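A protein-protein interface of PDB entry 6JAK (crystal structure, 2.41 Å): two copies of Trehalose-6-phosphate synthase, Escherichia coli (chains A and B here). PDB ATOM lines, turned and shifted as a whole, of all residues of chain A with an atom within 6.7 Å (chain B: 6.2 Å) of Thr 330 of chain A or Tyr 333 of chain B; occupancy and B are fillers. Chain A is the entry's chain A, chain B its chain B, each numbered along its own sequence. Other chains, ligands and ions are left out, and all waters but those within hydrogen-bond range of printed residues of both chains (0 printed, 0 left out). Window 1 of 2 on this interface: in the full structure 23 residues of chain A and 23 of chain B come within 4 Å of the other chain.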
ATOM      1  N   TYR A 276      23.236  28.558  20.876  1.00  0.00           N
ATOM      2  CA  TYR A 276      23.646  29.458  19.831  1.00  0.00           C
ATOM      3  C   TYR A 276      22.582  29.516  18.759  1.00  0.00           C
ATOM      4  O   TYR A 276      22.338  30.578  18.179  1.00  0.00           O
ATOM      5  CB  TYR A 276      24.990  29.035  19.258  1.00  0.00           C
ATOM      6  CG  TYR A 276      25.527  30.013  18.222  1.00  0.00           C
ATOM      7  CD1 TYR A 276      25.720  31.350  18.531  1.00  0.00           C
ATOM      8  CD2 TYR A 276      25.838  29.590  16.932  1.00  0.00           C
ATOM      9  CE1 TYR A 276      26.204  32.244  17.581  1.00  0.00           C
ATOM     10  CE2 TYR A 276      26.324  30.470  15.987  1.00  0.00           C
ATOM     11  CZ  TYR A 276      26.501  31.791  16.305  1.00  0.00           C
ATOM     12  OH  TYR A 276      27.015  32.653  15.355  1.00  0.00           O
ATOM     13  N   ILE A 290      28.170  38.325  13.950  1.00  0.00           N
ATOM     14  CA  ILE A 290      28.728  37.596  15.077  1.00  0.00           C
ATOM     15  C   ILE A 290      29.251  36.268  14.588  1.00  0.00           C
ATOM     16  O   ILE A 290      28.948  35.817  13.479  1.00  0.00           O
ATOM     17  CB  ILE A 290      27.712  37.348  16.218  1.00  0.00           C
ATOM     18  CG1 ILE A 290      26.611  36.371  15.808  1.00  0.00           C
ATOM     19  CG2 ILE A 290      27.071  38.649  16.718  1.00  0.00           C
ATOM     20  CD1 ILE A 290      25.765  35.988  17.039  1.00  0.00           C
ATOM     21  N   ARG A 291      29.997  35.607  15.464  1.00  0.00           N
ATOM     22  CA  ARG A 291      30.488  34.277  15.160  1.00  0.00           C
ATOM     23  C   ARG A 291      30.677  33.541  16.475  1.00  0.00           C
ATOM     24  O   ARG A 291      31.126  34.126  17.473  1.00  0.00           O
ATOM     25  CB  ARG A 291      31.803  34.315  14.377  1.00  0.00           C
ATOM     26  CG  ARG A 291      32.515  32.973  14.275  1.00  0.00           C
ATOM     27  CD  ARG A 291      33.859  33.151  13.612  1.00  0.00           C
ATOM     28  NE  ARG A 291      33.795  34.024  12.444  1.00  0.00           N
ATOM     29  CZ  ARG A 291      34.865  34.469  11.783  1.00  0.00           C
ATOM     30  NH1 ARG A 291      36.086  34.151  12.191  1.00  0.00           N
ATOM     31  NH2 ARG A 291      34.714  35.245  10.726  1.00  0.00           N
ATOM     32  N   TYR A 292      30.301  32.268  16.469  1.00  0.00           N
ATOM     33  CA  TYR A 292      30.575  31.337  17.551  1.00  0.00           C
ATOM     34  C   TYR A 292      31.670  30.396  17.060  1.00  0.00           C
ATOM     35  O   TYR A 292      31.519  29.766  16.006  1.00  0.00           O
ATOM     36  CB  TYR A 292      29.293  30.583  17.933  1.00  0.00           C
ATOM     37  CG  TYR A 292      29.468  29.555  19.011  1.00  0.00           C
ATOM     38  CD1 TYR A 292      30.529  29.630  19.906  1.00  0.00           C
ATOM     39  CD2 TYR A 292      28.614  28.476  19.111  1.00  0.00           C
ATOM     40  CE1 TYR A 292      30.711  28.667  20.883  1.00  0.00           C
ATOM     41  CE2 TYR A 292      28.797  27.502  20.083  1.00  0.00           C
ATOM     42  CZ  TYR A 292      29.838  27.609  20.962  1.00  0.00           C
ATOM     43  OH  TYR A 292      30.006  26.665  21.929  1.00  0.00           O
ATOM     44  N   ASN A 321      24.618  25.749  10.610  1.00  0.00           N
ATOM     45  CA  ASN A 321      25.106  26.513   9.477  1.00  0.00           C
ATOM     46  C   ASN A 321      24.199  26.319   8.267  1.00  0.00           C
ATOM     47  O   ASN A 321      23.940  27.267   7.527  1.00  0.00           O
ATOM     48  CB  ASN A 321      26.557  26.143   9.153  1.00  0.00           C
ATOM     49  CG  ASN A 321      27.552  26.689  10.172  1.00  0.00           C
ATOM     50  OD1 ASN A 321      27.327  27.736  10.805  1.00  0.00           O
ATOM     51  ND2 ASN A 321      28.649  25.959  10.364  1.00  0.00           N
ATOM     52  N   GLY A 325      23.188  29.925   7.907  1.00  0.00           N
ATOM     53  CA  GLY A 325      24.273  30.461   7.117  1.00  0.00           C
ATOM     54  C   GLY A 325      23.768  31.223   5.903  1.00  0.00           C
ATOM     55  O   GLY A 325      22.630  31.057   5.443  1.00  0.00           O
ATOM     56  N   GLN A 326      24.632  32.099   5.400  1.00  0.00           N
ATOM     57  CA  GLN A 326      24.420  32.876   4.189  1.00  0.00           C
ATOM     58  C   GLN A 326      25.552  32.543   3.235  1.00  0.00           C
ATOM     59  O   GLN A 326      26.543  31.907   3.604  1.00  0.00           O
ATOM     60  CB  GLN A 326      24.394  34.398   4.468  1.00  0.00           C
ATOM     61  CG  GLN A 326      23.146  34.967   5.189  1.00  0.00           C
ATOM     62  CD  GLN A 326      23.416  36.347   5.830  1.00  0.00           C
ATOM     63  OE1 GLN A 326      24.342  37.046   5.453  1.00  0.00           O
ATOM     64  NE2 GLN A 326      22.631  36.708   6.815  1.00  0.00           N
ATOM     65  N   LEU A 327      25.424  33.001   1.997  1.00  0.00           N
ATOM     66  CA  LEU A 327      26.500  32.772   1.042  1.00  0.00           C
ATOM     67  C   LEU A 327      27.816  33.407   1.468  1.00  0.00           C
ATOM     68  O   LEU A 327      28.876  32.935   1.044  1.00  0.00           O
ATOM     69  CB  LEU A 327      26.108  33.285  -0.325  1.00  0.00           C
ATOM     70  CG  LEU A 327      24.996  32.513  -1.009  1.00  0.00           C
ATOM     71  CD1 LEU A 327      24.398  33.452  -2.022  1.00  0.00           C
ATOM     72  CD2 LEU A 327      25.637  31.305  -1.700  1.00  0.00           C
ATOM     73  N   GLY A 328      27.781  34.414   2.331  1.00  0.00           N
ATOM     74  CA  GLY A 328      28.992  35.083   2.757  1.00  0.00           C
ATOM     75  C   GLY A 328      29.168  35.107   4.265  1.00  0.00           C
ATOM     76  O   GLY A 328      29.883  35.953   4.789  1.00  0.00           O
ATOM     77  N   TRP A 329      28.492  34.216   4.987  1.00  0.00           N
ATOM     78  CA  TRP A 329      28.581  34.246   6.440  1.00  0.00           C
ATOM     79  C   TRP A 329      28.306  32.868   6.988  1.00  0.00           C
ATOM     80  O   TRP A 329      27.200  32.339   6.820  1.00  0.00           O
ATOM     81  CB  TRP A 329      27.590  35.237   7.044  1.00  0.00           C
ATOM     82  CG  TRP A 329      27.547  35.260   8.553  1.00  0.00           C
ATOM     83  CD1 TRP A 329      28.549  35.652   9.399  1.00  0.00           C
ATOM     84  CD2 TRP A 329      26.431  34.907   9.399  1.00  0.00           C
ATOM     85  NE1 TRP A 329      28.124  35.566  10.710  1.00  0.00           N
ATOM     86  CE2 TRP A 329      26.838  35.106  10.741  1.00  0.00           C
ATOM     87  CE3 TRP A 329      25.136  34.452   9.152  1.00  0.00           C
ATOM     88  CZ2 TRP A 329      25.987  34.896  11.817  1.00  0.00           C
ATOM     89  CZ3 TRP A 329      24.297  34.236  10.226  1.00  0.00           C
ATOM     90  CH2 TRP A 329      24.724  34.468  11.539  1.00  0.00           C
ATOM     91  N   THR A 330      29.289  32.321   7.692  1.00  0.00           N
ATOM     92  CA  THR A 330      29.063  31.069   8.382  1.00  0.00           C
ATOM     93  C   THR A 330      28.957  31.377   9.870  1.00  0.00           C
ATOM     94  O   THR A 330      29.869  31.987  10.443  1.00  0.00           O
ATOM     95  CB  THR A 330      30.172  30.060   8.076  1.00  0.00           C
ATOM     96  OG1 THR A 330      30.044  29.673   6.703  1.00  0.00           O
ATOM     97  CG2 THR A 330      30.008  28.823   8.882  1.00  0.00           C
ATOM     98  N   PRO A 331      27.821  31.065  10.498  1.00  0.00           N
ATOM     99  CA  PRO A 331      27.642  31.424  11.920  1.00  0.00           C
ATOM    100  C   PRO A 331      28.574  30.694  12.888  1.00  0.00           C
ATOM    101  O   PRO A 331      29.022  31.299  13.870  1.00  0.00           O
ATOM    102  CB  PRO A 331      26.175  31.019  12.200  1.00  0.00           C
ATOM    103  CG  PRO A 331      25.525  30.854  10.878  1.00  0.00           C
ATOM    104  CD  PRO A 331      26.601  30.507   9.884  1.00  0.00           C
ATOM    105  N   LEU A 332      28.840  29.407  12.672  1.00  0.00           N
ATOM    106  CA  LEU A 332      29.438  28.536  13.682  1.00  0.00           C
ATOM    107  C   LEU A 332      30.689  27.886  13.122  1.00  0.00           C
ATOM    108  O   LEU A 332      30.606  27.084  12.186  1.00  0.00           O
ATOM    109  CB  LEU A 332      28.472  27.437  14.093  1.00  0.00           C
ATOM    110  CG  LEU A 332      28.595  26.781  15.480  1.00  0.00           C
ATOM    111  CD1 LEU A 332      27.348  25.889  15.813  1.00  0.00           C
ATOM    112  CD2 LEU A 332      29.892  26.030  15.685  1.00  0.00           C
ATOM    113  N   TYR A 333      31.824  28.174  13.730  1.00  0.00           N
ATOM    114  CA  TYR A 333      33.092  27.548  13.378  1.00  0.00           C
ATOM    115  C   TYR A 333      33.378  26.476  14.424  1.00  0.00           C
ATOM    116  O   TYR A 333      33.609  26.786  15.588  1.00  0.00           O
ATOM    117  CB  TYR A 333      34.224  28.563  13.365  1.00  0.00           C
ATOM    118  CG  TYR A 333      34.279  29.503  12.209  1.00  0.00           C
ATOM    119  CD1 TYR A 333      33.150  30.210  11.797  1.00  0.00           C
ATOM    120  CD2 TYR A 333      35.492  29.756  11.565  1.00  0.00           C
ATOM    121  CE1 TYR A 333      33.212  31.108  10.731  1.00  0.00           C
ATOM    122  CE2 TYR A 333      35.565  30.646  10.506  1.00  0.00           C
ATOM    123  CZ  TYR A 333      34.425  31.324  10.087  1.00  0.00           C
ATOM    124  OH  TYR A 333      34.521  32.206   9.023  1.00  0.00           O
ATOM    125  N   LEU B 251      34.229  38.644  -1.250  1.00  0.00           N
ATOM    126  CA  LEU B 251      35.114  37.551  -1.632  1.00  0.00           C
ATOM    127  C   LEU B 251      35.837  37.686  -2.958  1.00  0.00           C
ATOM    128  O   LEU B 251      35.642  36.849  -3.853  1.00  0.00           O
ATOM    129  CB  LEU B 251      34.353  36.255  -1.628  1.00  0.00           C
ATOM    130  CG  LEU B 251      33.860  36.073  -0.217  1.00  0.00           C
ATOM    131  CD1 LEU B 251      33.139  34.847  -0.308  1.00  0.00           C
ATOM    132  CD2 LEU B 251      35.005  35.962   0.804  1.00  0.00           C
ATOM    133  N   ARG B 291      36.482  28.052  -1.844  1.00  0.00           N
ATOM    134  CA  ARG B 291      35.295  27.708  -1.100  1.00  0.00           C
ATOM    135  C   ARG B 291      34.446  26.808  -1.970  1.00  0.00           C
ATOM    136  O   ARG B 291      34.357  27.009  -3.188  1.00  0.00           O
ATOM    137  CB  ARG B 291      34.525  28.953  -0.698  1.00  0.00           C
ATOM    138  CG  ARG B 291      33.162  28.653  -0.225  1.00  0.00           C
ATOM    139  CD  ARG B 291      32.460  29.938   0.073  1.00  0.00           C
ATOM    140  NE  ARG B 291      33.386  30.805   0.766  1.00  0.00           N
ATOM    141  CZ  ARG B 291      33.098  32.046   1.105  1.00  0.00           C
ATOM    142  NH1 ARG B 291      31.899  32.548   0.804  1.00  0.00           N
ATOM    143  NH2 ARG B 291      33.998  32.775   1.748  1.00  0.00           N
ATOM    144  N   TYR B 292      33.868  25.800  -1.336  1.00  0.00           N
ATOM    145  CA  TYR B 292      32.834  24.953  -1.922  1.00  0.00           C
ATOM    146  C   TYR B 292      31.496  25.321  -1.271  1.00  0.00           C
ATOM    147  O   TYR B 292      31.353  25.230  -0.050  1.00  0.00           O
ATOM    148  CB  TYR B 292      33.175  23.473  -1.713  1.00  0.00           C
ATOM    149  CG  TYR B 292      32.148  22.504  -2.235  1.00  0.00           C
ATOM    150  CD1 TYR B 292      31.273  22.845  -3.266  1.00  0.00           C
ATOM    151  CD2 TYR B 292      32.011  21.265  -1.664  1.00  0.00           C
ATOM    152  CE1 TYR B 292      30.315  21.943  -3.717  1.00  0.00           C
ATOM    153  CE2 TYR B 292      31.070  20.365  -2.106  1.00  0.00           C
ATOM    154  CZ  TYR B 292      30.232  20.697  -3.127  1.00  0.00           C
ATOM    155  OH  TYR B 292      29.310  19.736  -3.511  1.00  0.00           O
ATOM    156  N   THR B 293      30.531  25.740  -2.082  1.00  0.00           N
ATOM    157  CA  THR B 293      29.181  26.040  -1.624  1.00  0.00           C
ATOM    158  C   THR B 293      28.208  25.038  -2.218  1.00  0.00           C
ATOM    159  O   THR B 293      28.140  24.875  -3.435  1.00  0.00           O
ATOM    160  CB  THR B 293      28.749  27.467  -1.981  1.00  0.00           C
ATOM    161  OG1 THR B 293      29.586  28.398  -1.293  1.00  0.00           O
ATOM    162  CG2 THR B 293      27.311  27.710  -1.597  1.00  0.00           C
ATOM    163  N   GLN B 294      27.455  24.375  -1.358  1.00  0.00           N
ATOM    164  CA  GLN B 294      26.469  23.405  -1.788  1.00  0.00           C
ATOM    165  C   GLN B 294      25.111  23.906  -1.331  1.00  0.00           C
ATOM    166  O   GLN B 294      24.884  24.117  -0.134  1.00  0.00           O
ATOM    167  CB  GLN B 294      26.751  22.020  -1.210  1.00  0.00           C
ATOM    168  CG  GLN B 294      25.590  21.069  -1.527  1.00  0.00           C
ATOM    169  CD  GLN B 294      25.644  20.547  -2.948  1.00  0.00           C
ATOM    170  OE1 GLN B 294      26.672  20.028  -3.358  1.00  0.00           O
ATOM    171  NE2 GLN B 294      24.551  20.714  -3.724  1.00  0.00           N
ATOM    172  N   ILE B 295      24.237  24.169  -2.275  1.00  0.00           N
ATOM    173  CA  ILE B 295      22.883  24.547  -1.919  1.00  0.00           C
ATOM    174  C   ILE B 295      22.027  23.328  -2.149  1.00  0.00           C
ATOM    175  O   ILE B 295      22.093  22.703  -3.215  1.00  0.00           O
ATOM    176  CB  ILE B 295      22.374  25.746  -2.715  1.00  0.00           C
ATOM    177  CG1 ILE B 295      23.168  26.980  -2.319  1.00  0.00           C
ATOM    178  CG2 ILE B 295      20.900  25.946  -2.391  1.00  0.00           C
ATOM    179  CD1 ILE B 295      22.872  28.176  -3.140  1.00  0.00           C
ATOM    180  N   ASN B 321      34.739  20.740   7.728  1.00  0.00           N
ATOM    181  CA  ASN B 321      35.107  22.024   8.298  1.00  0.00           C
ATOM    182  C   ASN B 321      35.869  21.839   9.608  1.00  0.00           C
ATOM    183  O   ASN B 321      36.868  22.524   9.847  1.00  0.00           O
ATOM    184  CB  ASN B 321      33.867  22.891   8.492  1.00  0.00           C
ATOM    185  CG  ASN B 321      33.294  23.385   7.161  1.00  0.00           C
ATOM    186  OD1 ASN B 321      34.022  23.536   6.177  1.00  0.00           O
ATOM    187  ND2 ASN B 321      31.987  23.660   7.134  1.00  0.00           N
ATOM    188  N   THR B 330      36.571  28.942   6.439  1.00  0.00           N
ATOM    189  CA  THR B 330      35.775  27.720   6.416  1.00  0.00           C
ATOM    190  C   THR B 330      35.692  27.196   4.991  1.00  0.00           C
ATOM    191  O   THR B 330      35.211  27.907   4.104  1.00  0.00           O
ATOM    192  CB  THR B 330      34.371  27.920   6.977  1.00  0.00           C
ATOM    193  OG1 THR B 330      34.443  28.564   8.250  1.00  0.00           O
ATOM    194  CG2 THR B 330      33.733  26.570   7.164  1.00  0.00           C
ATOM    195  N   PRO B 331      36.141  25.968   4.751  1.00  0.00           N
ATOM    196  CA  PRO B 331      36.180  25.429   3.376  1.00  0.00           C
ATOM    197  C   PRO B 331      34.817  25.208   2.707  1.00  0.00           C
ATOM    198  O   PRO B 331      34.704  25.360   1.484  1.00  0.00           O
ATOM    199  CB  PRO B 331      36.885  24.072   3.557  1.00  0.00           C
ATOM    200  CG  PRO B 331      37.508  24.100   4.938  1.00  0.00           C
ATOM    201  CD  PRO B 331      36.716  25.055   5.764  1.00  0.00           C
ATOM    202  N   LEU B 332      33.802  24.775   3.447  1.00  0.00           N
ATOM    203  CA  LEU B 332      32.571  24.245   2.871  1.00  0.00           C
ATOM    204  C   LEU B 332      31.357  25.016   3.405  1.00  0.00           C
ATOM    205  O   LEU B 332      31.052  24.963   4.597  1.00  0.00           O
ATOM    206  CB  LEU B 332      32.453  22.756   3.223  1.00  0.00           C
ATOM    207  CG  LEU B 332      31.615  21.852   2.324  1.00  0.00           C
ATOM    208  CD1 LEU B 332      31.864  20.371   2.612  1.00  0.00           C
ATOM    209  CD2 LEU B 332      30.139  22.187   2.454  1.00  0.00           C
ATOM    210  N   TYR B 333      30.637  25.680   2.527  1.00  0.00           N
ATOM    211  CA  TYR B 333      29.390  26.345   2.875  1.00  0.00           C
ATOM    212  C   TYR B 333      28.252  25.452   2.403  1.00  0.00           C
ATOM    213  O   TYR B 333      28.028  25.314   1.196  1.00  0.00           O
ATOM    214  CB  TYR B 333      29.312  27.725   2.230  1.00  0.00           C
ATOM    215  CG  TYR B 333      30.132  28.795   2.899  1.00  0.00           C
ATOM    216  CD1 TYR B 333      31.461  28.579   3.248  1.00  0.00           C
ATOM    217  CD2 TYR B 333      29.589  30.037   3.136  1.00  0.00           C
ATOM    218  CE1 TYR B 333      32.203  29.555   3.858  1.00  0.00           C
ATOM    219  CE2 TYR B 333      30.316  31.024   3.728  1.00  0.00           C
ATOM    220  CZ  TYR B 333      31.619  30.780   4.095  1.00  0.00           C
ATOM    221  OH  TYR B 333      32.322  31.786   4.688  1.00  0.00           O
ATOM    222  N   TYR B 334      27.535  24.850   3.339  1.00  0.00           N
ATOM    223  CA  TYR B 334      26.395  23.979   3.030  1.00  0.00           C
ATOM    224  C   TYR B 334      25.124  24.718   3.392  1.00  0.00           C
ATOM    225  O   TYR B 334      24.987  25.193   4.526  1.00  0.00           O
ATOM    226  CB  TYR B 334      26.502  22.652   3.778  1.00  0.00           C
ATOM    227  CG  TYR B 334      25.211  21.866   3.887  1.00  0.00           C
ATOM    228  CD1 TYR B 334      24.584  21.372   2.758  1.00  0.00           C
ATOM    229  CD2 TYR B 334      24.630  21.588   5.142  1.00  0.00           C
ATOM    230  CE1 TYR B 334      23.401  20.636   2.854  1.00  0.00           C
ATOM    231  CE2 TYR B 334      23.448  20.856   5.246  1.00  0.00           C
ATOM    232  CZ  TYR B 334      22.841  20.376   4.092  1.00  0.00           C
ATOM    233  OH  TYR B 334      21.668  19.645   4.128  1.00  0.00           O
ATOM    234  N   LEU B 335      24.227  24.891   2.420  1.00  0.00           N
ATOM    235  CA  LEU B 335      23.017  25.672   2.674  1.00  0.00           C
ATOM    236  C   LEU B 335      21.783  24.847   2.372  1.00  0.00           C
ATOM    237  O   LEU B 335      21.542  24.439   1.232  1.00  0.00           O
ATOM    238  CB  LEU B 335      23.000  26.998   1.901  1.00  0.00           C
ATOM    239  CG  LEU B 335      24.152  27.912   2.326  1.00  0.00           C
ATOM    240  CD1 LEU B 335      24.258  29.148   1.443  1.00  0.00           C
ATOM    241  CD2 LEU B 335      24.019  28.265   3.823  1.00  0.00           C
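Of chain B, only Tyr 333 comes within 4 Å of Thr 330 of chain A.
Of chain A, only Gln 326 (3.6 Å), Leu 327 (3.6 Å), Trp 329 (3.9 Å) and Thr 330 (3.2 Å) come within 4 Å of Tyr 333 of chain B.
Printed residues of chain B within 4 Å of Gly 325 of chain A: Leu 335 (3.5 Å).
Printed residues of chain A within 4 Å of Thr 330 of chain B: Tyr 333 (3.3 Å).
Of the printed residues of chain A, Tyr 334 of chain B touches Asn 321 (3.8 Å).
Of the printed residues of chain B, Tyr 333 of chain A touches Thr 330 (3.3 Å).
Of the printed residues of chain B, Trp 329 of chain A touches Tyr 333.
The nearest residue of chain B that does not touch Thr 330 of chain A is Thr 330 of chain B (4.5 Å).
The nearest residue of chain A that does not touch Tyr 333 of chain B is Gly 328 of chain A (4.3 Å).
The nearest printed residue of chain A that does not touch Tyr 334 of chain B is Gly 325 of chain A (5.9 Å).
The backbone carbonyl oxygen (O) of Leu 327 of chain A lies within hydrogen-bond range of the guanidinium group (NH1) of Arg 291 of chain B (3.1 Å).
The indole nitrogen of Trp 329 of chain A sits at hydrogen-bond distance from the backbone carbonyl oxygen of Ile 290 of chain A (2.9 Å).
OH of Tyr 333 of chain A lies within hydrogen-bond range of NH2 of Arg 291 of chain A (3.5 Å).
O of Tyr 292 of chain A is in hydrogen-bond range of N of Tyr 333 of chain A, at 2.8 Å.
ND2 of Asn 321 of chain A sits at hydrogen-bond distance from O of Leu 332 of chain A, 2.9 Å away.
The backbone NH of Tyr 333 of chain B sits at hydrogen-bond distance from the backbone carbonyl oxygen of Tyr 292 of chain B, 2.7 Å away.
The backbone NH (N) of Gln 294 of chain B is in hydrogen-bond range of the backbone carbonyl oxygen (O) of Tyr 333 of chain B (2.8 Å).
Among the printed residues, merely in contact across the chains: Asn 321 of chain A with Tyr 334 of chain B (3.8 Å), Asn 321 of chain A with Leu 335 of chain B (3.8 Å), Gly 325 of chain A with Leu 335 of chain B (3.5 Å), Gln 326 of chain A with Tyr 333 of chain B (3.6 Å), Leu 327 of chain A with Thr 293 of chain B (3.97 Å), Leu 327 of chain A with Tyr 333 of chain B (3.6 Å), Trp 329 of chain A with Tyr 333 of chain B (3.9 Å), Thr 330 of chain A with Tyr 333 of chain B (3.2 Å) and Tyr 333 of chain A with Thr 330 of chain B (3.3 Å).
Thr 330 of chain A touches Tyr 333 of chain B, and with the chains exchanged Tyr 333 of chain A touches Thr 330 of chain B.
7 positions are printed for both chains.
Printed residues of chain A that touch a printed residue of chain B: Asn 321, Gly 325, Gln 326, Leu 327, Trp 329, Thr 330 and Tyr 333.
Hydrophobic or aromatic side chains of chain A within 4 Å of the printed part of chain B: Leu 327 and Tyr 333.
Of the 13 printed residues of chain B, 6 touch a printed residue of chain A.
Hydrophobic or aromatic side chains of chain B within 4 Å of the printed part of chain A: Tyr 333 and Leu 335.
Among the printed residues, 10 pairs touch across the chains.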
